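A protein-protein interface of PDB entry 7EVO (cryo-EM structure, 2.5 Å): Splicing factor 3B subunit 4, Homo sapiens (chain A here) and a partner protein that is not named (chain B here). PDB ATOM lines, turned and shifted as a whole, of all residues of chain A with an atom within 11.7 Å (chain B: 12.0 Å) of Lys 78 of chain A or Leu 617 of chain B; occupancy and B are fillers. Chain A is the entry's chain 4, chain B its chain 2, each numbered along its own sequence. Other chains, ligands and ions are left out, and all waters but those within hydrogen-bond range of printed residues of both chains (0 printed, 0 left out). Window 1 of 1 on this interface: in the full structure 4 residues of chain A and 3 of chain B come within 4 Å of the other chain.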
ATOM      1  N   GLY A  18      22.182  35.800 -12.021  1.00  0.00           N
ATOM      2  CA  GLY A  18      21.863  37.057 -12.676  1.00  0.00           C
ATOM      3  C   GLY A  18      21.624  36.846 -14.155  1.00  0.00           C
ATOM      4  O   GLY A  18      22.219  35.970 -14.784  1.00  0.00           O
ATOM      5  N   GLY A  19      20.737  37.670 -14.706  1.00  0.00           N
ATOM      6  CA  GLY A  19      20.394  37.574 -16.110  1.00  0.00           C
ATOM      7  C   GLY A  19      19.287  36.580 -16.387  1.00  0.00           C
ATOM      8  O   GLY A  19      19.473  35.633 -17.157  1.00  0.00           O
ATOM      9  N   LEU A  20      18.131  36.776 -15.758  1.00  0.00           N
ATOM     10  CA  LEU A  20      16.972  35.915 -15.941  1.00  0.00           C
ATOM     11  C   LEU A  20      15.896  36.673 -16.702  1.00  0.00           C
ATOM     12  O   LEU A  20      15.563  37.811 -16.350  1.00  0.00           O
ATOM     13  N   ASP A  21      15.352  36.044 -17.741  1.00  0.00           N
ATOM     14  CA  ASP A  21      14.319  36.653 -18.564  1.00  0.00           C
ATOM     15  C   ASP A  21      12.943  36.363 -17.962  1.00  0.00           C
ATOM     16  O   ASP A  21      12.822  35.858 -16.845  1.00  0.00           O
ATOM     17  N   GLU A  22      11.885  36.683 -18.711  1.00  0.00           N
ATOM     18  CA  GLU A  22      10.527  36.450 -18.239  1.00  0.00           C
ATOM     19  C   GLU A  22      10.120  34.984 -18.308  1.00  0.00           C
ATOM     20  O   GLU A  22       9.166  34.589 -17.634  1.00  0.00           O
ATOM     21  N   LYS A  23      10.818  34.174 -19.109  1.00  0.00           N
ATOM     22  CA  LYS A  23      10.480  32.755 -19.198  1.00  0.00           C
ATOM     23  C   LYS A  23      10.955  31.987 -17.972  1.00  0.00           C
ATOM     24  O   LYS A  23      10.357  30.963 -17.614  1.00  0.00           O
ATOM     25  N   VAL A  24      12.020  32.455 -17.319  1.00  0.00           N
ATOM     26  CA  VAL A  24      12.514  31.795 -16.117  1.00  0.00           C
ATOM     27  C   VAL A  24      11.603  32.122 -14.943  1.00  0.00           C
ATOM     28  O   VAL A  24      11.082  33.241 -14.829  1.00  0.00           O
ATOM     29  N   SER A  25      11.404  31.145 -14.064  1.00  0.00           N
ATOM     30  CA  SER A  25      10.527  31.287 -12.911  1.00  0.00           C
ATOM     31  C   SER A  25      11.249  30.786 -11.663  1.00  0.00           C
ATOM     32  O   SER A  25      12.423  30.409 -11.705  1.00  0.00           O
ATOM     33  N   LEU A  28      11.575  26.954 -11.895  1.00  0.00           N
ATOM     34  CA  LEU A  28      12.385  26.636 -13.068  1.00  0.00           C
ATOM     35  C   LEU A  28      13.877  26.717 -12.771  1.00  0.00           C
ATOM     36  O   LEU A  28      14.647  25.881 -13.262  1.00  0.00           O
ATOM     37  N   LEU A  32      16.452  23.631 -12.948  1.00  0.00           N
ATOM     38  CA  LEU A  32      17.671  23.696 -13.750  1.00  0.00           C
ATOM     39  C   LEU A  32      18.920  23.503 -12.898  1.00  0.00           C
ATOM     40  O   LEU A  32      19.922  22.969 -13.384  1.00  0.00           O
ATOM     41  N   ALA A  70      27.677  24.718  -9.257  1.00  0.00           N
ATOM     42  CA  ALA A  70      26.672  25.451 -10.022  1.00  0.00           C
ATOM     43  C   ALA A  70      27.220  26.779 -10.531  1.00  0.00           C
ATOM     44  O   ALA A  70      26.826  27.250 -11.603  1.00  0.00           O
ATOM     45  N   ILE A  73      29.582  25.749 -13.443  1.00  0.00           N
ATOM     46  CA  ILE A  73      28.931  25.049 -14.543  1.00  0.00           C
ATOM     47  C   ILE A  73      27.958  25.959 -15.285  1.00  0.00           C
ATOM     48  O   ILE A  73      27.934  25.983 -16.517  1.00  0.00           O
ATOM     49  N   MET A  74      27.145  26.716 -14.550  1.00  0.00           N
ATOM     50  CA  MET A  74      26.133  27.581 -15.141  1.00  0.00           C
ATOM     51  C   MET A  74      26.616  29.015 -15.326  1.00  0.00           C
ATOM     52  O   MET A  74      25.802  29.943 -15.285  1.00  0.00           O
ATOM     53  N   ASN A  75      27.916  29.216 -15.528  1.00  0.00           N
ATOM     54  CA  ASN A  75      28.473  30.548 -15.728  1.00  0.00           C
ATOM     55  C   ASN A  75      28.394  30.925 -17.200  1.00  0.00           C
ATOM     56  O   ASN A  75      28.794  30.138 -18.067  1.00  0.00           O
ATOM     57  N   MET A  76      27.873  32.134 -17.466  1.00  0.00           N
ATOM     58  CA  MET A  76      27.734  32.713 -18.812  1.00  0.00           C
ATOM     59  C   MET A  76      26.901  31.827 -19.736  1.00  0.00           C
ATOM     60  O   MET A  76      27.210  31.665 -20.918  1.00  0.00           O
ATOM     61  N   ILE A  77      25.833  31.246 -19.192  1.00  0.00           N
ATOM     62  CA  ILE A  77      24.957  30.394 -19.987  1.00  0.00           C
ATOM     63  C   ILE A  77      23.858  31.236 -20.628  1.00  0.00           C
ATOM     64  O   ILE A  77      23.534  32.338 -20.182  1.00  0.00           O
ATOM     65  N   LYS A  78      23.277  30.701 -21.700  1.00  0.00           N
ATOM     66  CA  LYS A  78      22.202  31.369 -22.431  1.00  0.00           C
ATOM     67  C   LYS A  78      20.883  30.727 -22.009  1.00  0.00           C
ATOM     68  O   LYS A  78      20.423  29.754 -22.608  1.00  0.00           O
ATOM     69  N   LEU A  79      20.273  31.281 -20.965  1.00  0.00           N
ATOM     70  CA  LEU A  79      19.019  30.772 -20.422  1.00  0.00           C
ATOM     71  C   LEU A  79      17.905  31.746 -20.775  1.00  0.00           C
ATOM     72  O   LEU A  79      17.983  32.929 -20.425  1.00  0.00           O
ATOM     73  N   TYR A  80      16.882  31.239 -21.477  1.00  0.00           N
ATOM     74  CA  TYR A  80      15.702  31.996 -21.922  1.00  0.00           C
ATOM     75  C   TYR A  80      16.076  33.207 -22.773  1.00  0.00           C
ATOM     76  O   TYR A  80      15.417  34.248 -22.713  1.00  0.00           O
ATOM     77  N   GLY A  81      17.127  33.078 -23.577  1.00  0.00           N
ATOM     78  CA  GLY A  81      17.636  34.199 -24.346  1.00  0.00           C
ATOM     79  C   GLY A  81      18.263  35.280 -23.491  1.00  0.00           C
ATOM     80  O   GLY A  81      18.194  36.463 -23.844  1.00  0.00           O
ATOM     81  N   LYS A  82      18.879  34.900 -22.369  1.00  0.00           N
ATOM     82  CA  LYS A  82      19.439  35.860 -21.435  1.00  0.00           C
ATOM     83  C   LYS A  82      20.753  35.327 -20.881  1.00  0.00           C
ATOM     84  O   LYS A  82      20.877  34.113 -20.662  1.00  0.00           O
ATOM     85  N   PRO A  83      21.747  36.197 -20.652  1.00  0.00           N
ATOM     86  CA  PRO A  83      23.023  35.728 -20.097  1.00  0.00           C
ATOM     87  C   PRO A  83      22.947  35.424 -18.608  1.00  0.00           C
ATOM     88  O   PRO A  83      23.324  36.248 -17.769  1.00  0.00           O
ATOM     89  CB  PRO A  83      23.979  36.891 -20.391  1.00  0.00           C
ATOM     90  CG  PRO A  83      23.093  38.095 -20.462  1.00  0.00           C
ATOM     91  CD  PRO A  83      21.792  37.620 -21.034  1.00  0.00           C
ATOM     92  N   ILE A  84      22.467  34.227 -18.271  1.00  0.00           N
ATOM     93  CA  ILE A  84      22.357  33.839 -16.869  1.00  0.00           C
ATOM     94  C   ILE A  84      23.706  33.339 -16.372  1.00  0.00           C
ATOM     95  O   ILE A  84      24.388  32.555 -17.045  1.00  0.00           O
ATOM     96  N   ARG A  85      24.096  33.793 -15.184  1.00  0.00           N
ATOM     97  CA  ARG A  85      25.365  33.395 -14.591  1.00  0.00           C
ATOM     98  C   ARG A  85      25.209  33.334 -13.080  1.00  0.00           C
ATOM     99  O   ARG A  85      24.541  34.183 -12.484  1.00  0.00           O
ATOM    100  N   VAL A  86      25.832  32.330 -12.469  1.00  0.00           N
ATOM    101  CA  VAL A  86      25.769  32.112 -11.030  1.00  0.00           C
ATOM    102  C   VAL A  86      27.085  32.553 -10.409  1.00  0.00           C
ATOM    103  O   VAL A  86      28.161  32.309 -10.967  1.00  0.00           O
ATOM    104  N   ASP A 108      26.651  42.340 -18.749  1.00  0.00           N
ATOM    105  CA  ASP A 108      26.400  40.966 -18.334  1.00  0.00           C
ATOM    106  C   ASP A 108      26.967  40.723 -16.936  1.00  0.00           C
ATOM    107  O   ASP A 108      28.052  41.215 -16.611  1.00  0.00           O
ATOM    108  N   PRO A 109      26.256  39.970 -16.088  1.00  0.00           N
ATOM    109  CA  PRO A 109      26.772  39.691 -14.739  1.00  0.00           C
ATOM    110  C   PRO A 109      27.855  38.625 -14.694  1.00  0.00           C
ATOM    111  O   PRO A 109      28.422  38.396 -13.617  1.00  0.00           O
ATOM    112  CB  PRO A 109      25.521  39.226 -13.983  1.00  0.00           C
ATOM    113  CG  PRO A 109      24.656  38.633 -15.037  1.00  0.00           C
ATOM    114  CD  PRO A 109      24.891  39.449 -16.279  1.00  0.00           C
ATOM    115  N   GLU A 110      28.158  37.966 -15.817  1.00  0.00           N
ATOM    116  CA  GLU A 110      29.192  36.938 -15.826  1.00  0.00           C
ATOM    117  C   GLU A 110      30.597  37.523 -15.751  1.00  0.00           C
ATOM    118  O   GLU A 110      31.527  36.814 -15.356  1.00  0.00           O
ATOM    119  N   LEU A 167      28.845  42.383 -26.610  1.00  0.00           N
ATOM    120  CA  LEU A 167      29.403  41.700 -25.451  1.00  0.00           C
ATOM    121  C   LEU A 167      28.836  40.288 -25.349  1.00  0.00           C
ATOM    122  O   LEU A 167      28.211  39.796 -26.295  1.00  0.00           O
ATOM    123  N   CYS A 168      29.052  39.630 -24.210  1.00  0.00           N
ATOM    124  CA  CYS A 168      28.591  38.259 -24.024  1.00  0.00           C
ATOM    125  C   CYS A 168      27.078  38.208 -23.849  1.00  0.00           C
ATOM    126  O   CYS A 168      26.579  38.208 -22.717  1.00  0.00           O
ATOM    127  N   ASN A 169      26.359  38.185 -24.981  1.00  0.00           N
ATOM    128  CA  ASN A 169      24.894  38.073 -25.055  1.00  0.00           C
ATOM    129  C   ASN A 169      24.188  39.213 -24.318  1.00  0.00           C
ATOM    130  O   ASN A 169      23.118  39.029 -23.734  1.00  0.00           O
ATOM    131  N   ARG A 170      24.788  40.401 -24.353  1.00  0.00           N
ATOM    132  CA  ARG A 170      24.215  41.570 -23.697  1.00  0.00           C
ATOM    133  C   ARG A 170      24.694  42.844 -24.383  1.00  0.00           C
ATOM    134  O   ARG A 170      25.889  43.160 -24.337  1.00  0.00           O
ATOM    135  N   LEU B 609      14.706  18.932 -18.413  1.00  0.00           N
ATOM    136  CA  LEU B 609      14.379  20.324 -18.685  1.00  0.00           C
ATOM    137  C   LEU B 609      13.031  20.404 -19.390  1.00  0.00           C
ATOM    138  O   LEU B 609      12.643  19.494 -20.124  1.00  0.00           O
ATOM    139  N   SER B 610      12.326  21.508 -19.153  1.00  0.00           N
ATOM    140  CA  SER B 610      11.030  21.714 -19.776  1.00  0.00           C
ATOM    141  C   SER B 610      11.192  22.095 -21.244  1.00  0.00           C
ATOM    142  O   SER B 610      12.262  22.519 -21.691  1.00  0.00           O
ATOM    143  N   ASP B 611      10.103  21.937 -22.000  1.00  0.00           N
ATOM    144  CA  ASP B 611      10.137  22.263 -23.422  1.00  0.00           C
ATOM    145  C   ASP B 611      10.110  23.767 -23.658  1.00  0.00           C
ATOM    146  O   ASP B 611      10.727  24.252 -24.615  1.00  0.00           O
ATOM    147  N   GLU B 612       9.414  24.518 -22.798  1.00  0.00           N
ATOM    148  CA  GLU B 612       9.332  25.967 -22.968  1.00  0.00           C
ATOM    149  C   GLU B 612      10.663  26.639 -22.655  1.00  0.00           C
ATOM    150  O   GLU B 612      11.081  27.559 -23.367  1.00  0.00           O
ATOM    151  N   LEU B 613      11.349  26.182 -21.603  1.00  0.00           N
ATOM    152  CA  LEU B 613      12.660  26.732 -21.273  1.00  0.00           C
ATOM    153  C   LEU B 613      13.707  26.352 -22.311  1.00  0.00           C
ATOM    154  O   LEU B 613      14.600  27.154 -22.611  1.00  0.00           O
ATOM    155  N   ARG B 614      13.608  25.148 -22.881  1.00  0.00           N
ATOM    156  CA  ARG B 614      14.534  24.746 -23.935  1.00  0.00           C
ATOM    157  C   ARG B 614      14.253  25.485 -25.238  1.00  0.00           C
ATOM    158  O   ARG B 614      15.179  25.725 -26.022  1.00  0.00           O
ATOM    159  N   ILE B 615      12.996  25.850 -25.486  1.00  0.00           N
ATOM    160  CA  ILE B 615      12.679  26.631 -26.677  1.00  0.00           C
ATOM    161  C   ILE B 615      13.094  28.090 -26.499  1.00  0.00           C
ATOM    162  O   ILE B 615      13.519  28.738 -27.463  1.00  0.00           O
ATOM    163  N   SER B 616      12.979  28.626 -25.284  1.00  0.00           N
ATOM    164  CA  SER B 616      13.372  30.012 -25.043  1.00  0.00           C
ATOM    165  C   SER B 616      14.882  30.173 -24.935  1.00  0.00           C
ATOM    166  O   SER B 616      15.410  31.242 -25.265  1.00  0.00           O
ATOM    167  N   LEU B 617      15.592  29.139 -24.482  1.00  0.00           N
ATOM    168  CA  LEU B 617      17.040  29.218 -24.336  1.00  0.00           C
ATOM    169  C   LEU B 617      17.783  29.077 -25.659  1.00  0.00           C
ATOM    170  O   LEU B 617      18.981  29.373 -25.710  1.00  0.00           O
ATOM    171  N   GLY B 618      17.114  28.636 -26.720  1.00  0.00           N
ATOM    172  CA  GLY B 618      17.770  28.479 -28.003  1.00  0.00           C
ATOM    173  C   GLY B 618      18.442  27.141 -28.208  1.00  0.00           C
ATOM    174  O   GLY B 618      19.391  27.046 -28.990  1.00  0.00           O
ATOM    175  N   MET B 619      17.973  26.095 -27.522  1.00  0.00           N
ATOM    176  CA  MET B 619      18.554  24.766 -27.658  1.00  0.00           C
ATOM    177  C   MET B 619      17.726  23.930 -28.617  1.00  0.00           C
ATOM    178  O   MET B 619      16.496  23.859 -28.463  1.00  0.00           O
ATOM    179  N   PRO B 620      18.342  23.292 -29.609  1.00  0.00           N
ATOM    180  CA  PRO B 620      17.581  22.471 -30.555  1.00  0.00           C
ATOM    181  C   PRO B 620      17.156  21.147 -29.932  1.00  0.00           C
ATOM    182  O   PRO B 620      17.558  20.781 -28.827  1.00  0.00           O
ATOM    183  CB  PRO B 620      18.571  22.249 -31.702  1.00  0.00           C
ATOM    184  CG  PRO B 620      19.908  22.331 -31.052  1.00  0.00           C
ATOM    185  CD  PRO B 620      19.773  23.353 -29.956  1.00  0.00           C
ATOM    186  N   VAL B 621      16.315  20.423 -30.678  1.00  0.00           N
ATOM    187  CA  VAL B 621      15.821  19.140 -30.197  1.00  0.00           C
ATOM    188  C   VAL B 621      16.898  18.069 -30.352  1.00  0.00           C
ATOM    189  O   VAL B 621      17.905  18.246 -31.049  1.00  0.00           O
ATOM    190  N   PRO B 629      25.028  18.501 -26.944  1.00  0.00           N
ATOM    191  CA  PRO B 629      24.995  18.689 -25.495  1.00  0.00           C
ATOM    192  C   PRO B 629      24.455  20.061 -25.136  1.00  0.00           C
ATOM    193  O   PRO B 629      24.478  20.986 -25.965  1.00  0.00           O
ATOM    194  CB  PRO B 629      26.473  18.554 -25.095  1.00  0.00           C
ATOM    195  CG  PRO B 629      27.201  19.085 -26.279  1.00  0.00           C
ATOM    196  CD  PRO B 629      26.385  18.696 -27.491  1.00  0.00           C
ATOM    197  N   PRO B 630      23.947  20.235 -23.920  1.00  0.00           N
ATOM    198  CA  PRO B 630      23.645  21.582 -23.425  1.00  0.00           C
ATOM    199  C   PRO B 630      24.928  22.344 -23.144  1.00  0.00           C
ATOM    200  O   PRO B 630      25.993  21.731 -22.983  1.00  0.00           O
ATOM    201  CB  PRO B 630      22.850  21.308 -22.135  1.00  0.00           C
ATOM    202  CG  PRO B 630      23.279  19.957 -21.706  1.00  0.00           C
ATOM    203  CD  PRO B 630      23.532  19.189 -22.968  1.00  0.00           C
ATOM    204  N   PRO B 631      24.882  23.684 -23.094  1.00  0.00           N
ATOM    205  CA  PRO B 631      26.114  24.448 -22.828  1.00  0.00           C
ATOM    206  C   PRO B 631      26.653  24.302 -21.410  1.00  0.00           C
ATOM    207  O   PRO B 631      27.796  24.710 -21.163  1.00  0.00           O
ATOM    208  CB  PRO B 631      25.699  25.897 -23.115  1.00  0.00           C
ATOM    209  CG  PRO B 631      24.229  25.914 -22.922  1.00  0.00           C
ATOM    210  CD  PRO B 631      23.745  24.576 -23.389  1.00  0.00           C
ATOM    211  N   TRP B 632      25.879  23.746 -20.478  1.00  0.00           N
ATOM    212  CA  TRP B 632      26.395  23.427 -19.154  1.00  0.00           C
ATOM    213  C   TRP B 632      27.090  22.072 -19.104  1.00  0.00           C
ATOM    214  O   TRP B 632      27.717  21.752 -18.088  1.00  0.00           O
ATOM    215  N   LEU B 633      26.994  21.272 -20.168  1.00  0.00           N
ATOM    216  CA  LEU B 633      27.631  19.962 -20.210  1.00  0.00           C
ATOM    217  C   LEU B 633      29.093  20.027 -20.628  1.00  0.00           C
ATOM    218  O   LEU B 633      29.848  19.087 -20.355  1.00  0.00           O
ATOM    219  N   ILE B 634      29.510  21.117 -21.278  1.00  0.00           N
ATOM    220  CA  ILE B 634      30.909  21.262 -21.669  1.00  0.00           C
ATOM    221  C   ILE B 634      31.789  21.463 -20.441  1.00  0.00           C
ATOM    222  O   ILE B 634      32.906  20.937 -20.368  1.00  0.00           O
ATOM    223  N   ALA B 635      31.290  22.204 -19.447  1.00  0.00           N
ATOM    224  CA  ALA B 635      32.027  22.373 -18.200  1.00  0.00           C
ATOM    225  C   ALA B 635      32.096  21.074 -17.405  1.00  0.00           C
ATOM    226  O   ALA B 635      33.098  20.816 -16.732  1.00  0.00           O
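The backbone NH (N) of Gly 81 of chain A sits at hydrogen-bond distance from the backbone carbonyl oxygen (O) of Ser 616 of chain B. O of Leu 617 of chain B sits close to O of Lys 78 of chain A (3.4 Å).
Trp 632 of chain B touches Ile 73 of chain A (CA to O, 3.98 Å). O of Ser 616 of chain B touches C of Tyr 80 of chain A (3.2 Å). CA of Leu 617 of chain B touches N of Tyr 80 of chain A (3.5 Å). Gly 81 of chain A touches Leu 617 of chain B.
Of the printed residues of chain B, Ile 73 of chain A touches Trp 632. Met 76 of chain A touches none of the printed residues of chain B. No residue of chain B comes within 4 Å of Ile 77 of chain A. Of the printed residues of chain B, Lys 78 of chain A touches Leu 617. Leu 79 of chain A touches none of the printed residues of chain B. Of chain B, only Ser 616 and Leu 617 come within 4 Å of Tyr 80 of chain A. No residue of chain B comes within 4 Å of Pro 83 of chain A. No residue of chain A comes within 4 Å of Leu 613 of chain B. No residue of chain A comes within 4 Å of Ile 615 of chain B. Ser 616 of chain B touches two residues of chain A. Of chain A, only Lys 78 (3.4 Å), Tyr 80 (3.5 Å) and Gly 81 (3.9 Å) come within 4 Å of Leu 617 of chain B. No residue of chain A comes within 4 Å of Met 619 of chain B. Printed residues of chain A within 4 Å of Trp 632 of chain B: Ile 73. The nearest residue of chain B that does not touch Lys 78 of chain A is Pro 631 of chain B (5.0 Å).
Of the 32 printed residues of chain A, 4 touch a printed residue of chain B. Printed residues of chain A that touch a printed residue of chain B: Ile 73, Lys 78, Tyr 80 and Gly 81. Printed residues of chain B that touch a printed residue of chain A: Ser 616, Leu 617 and Trp 632.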
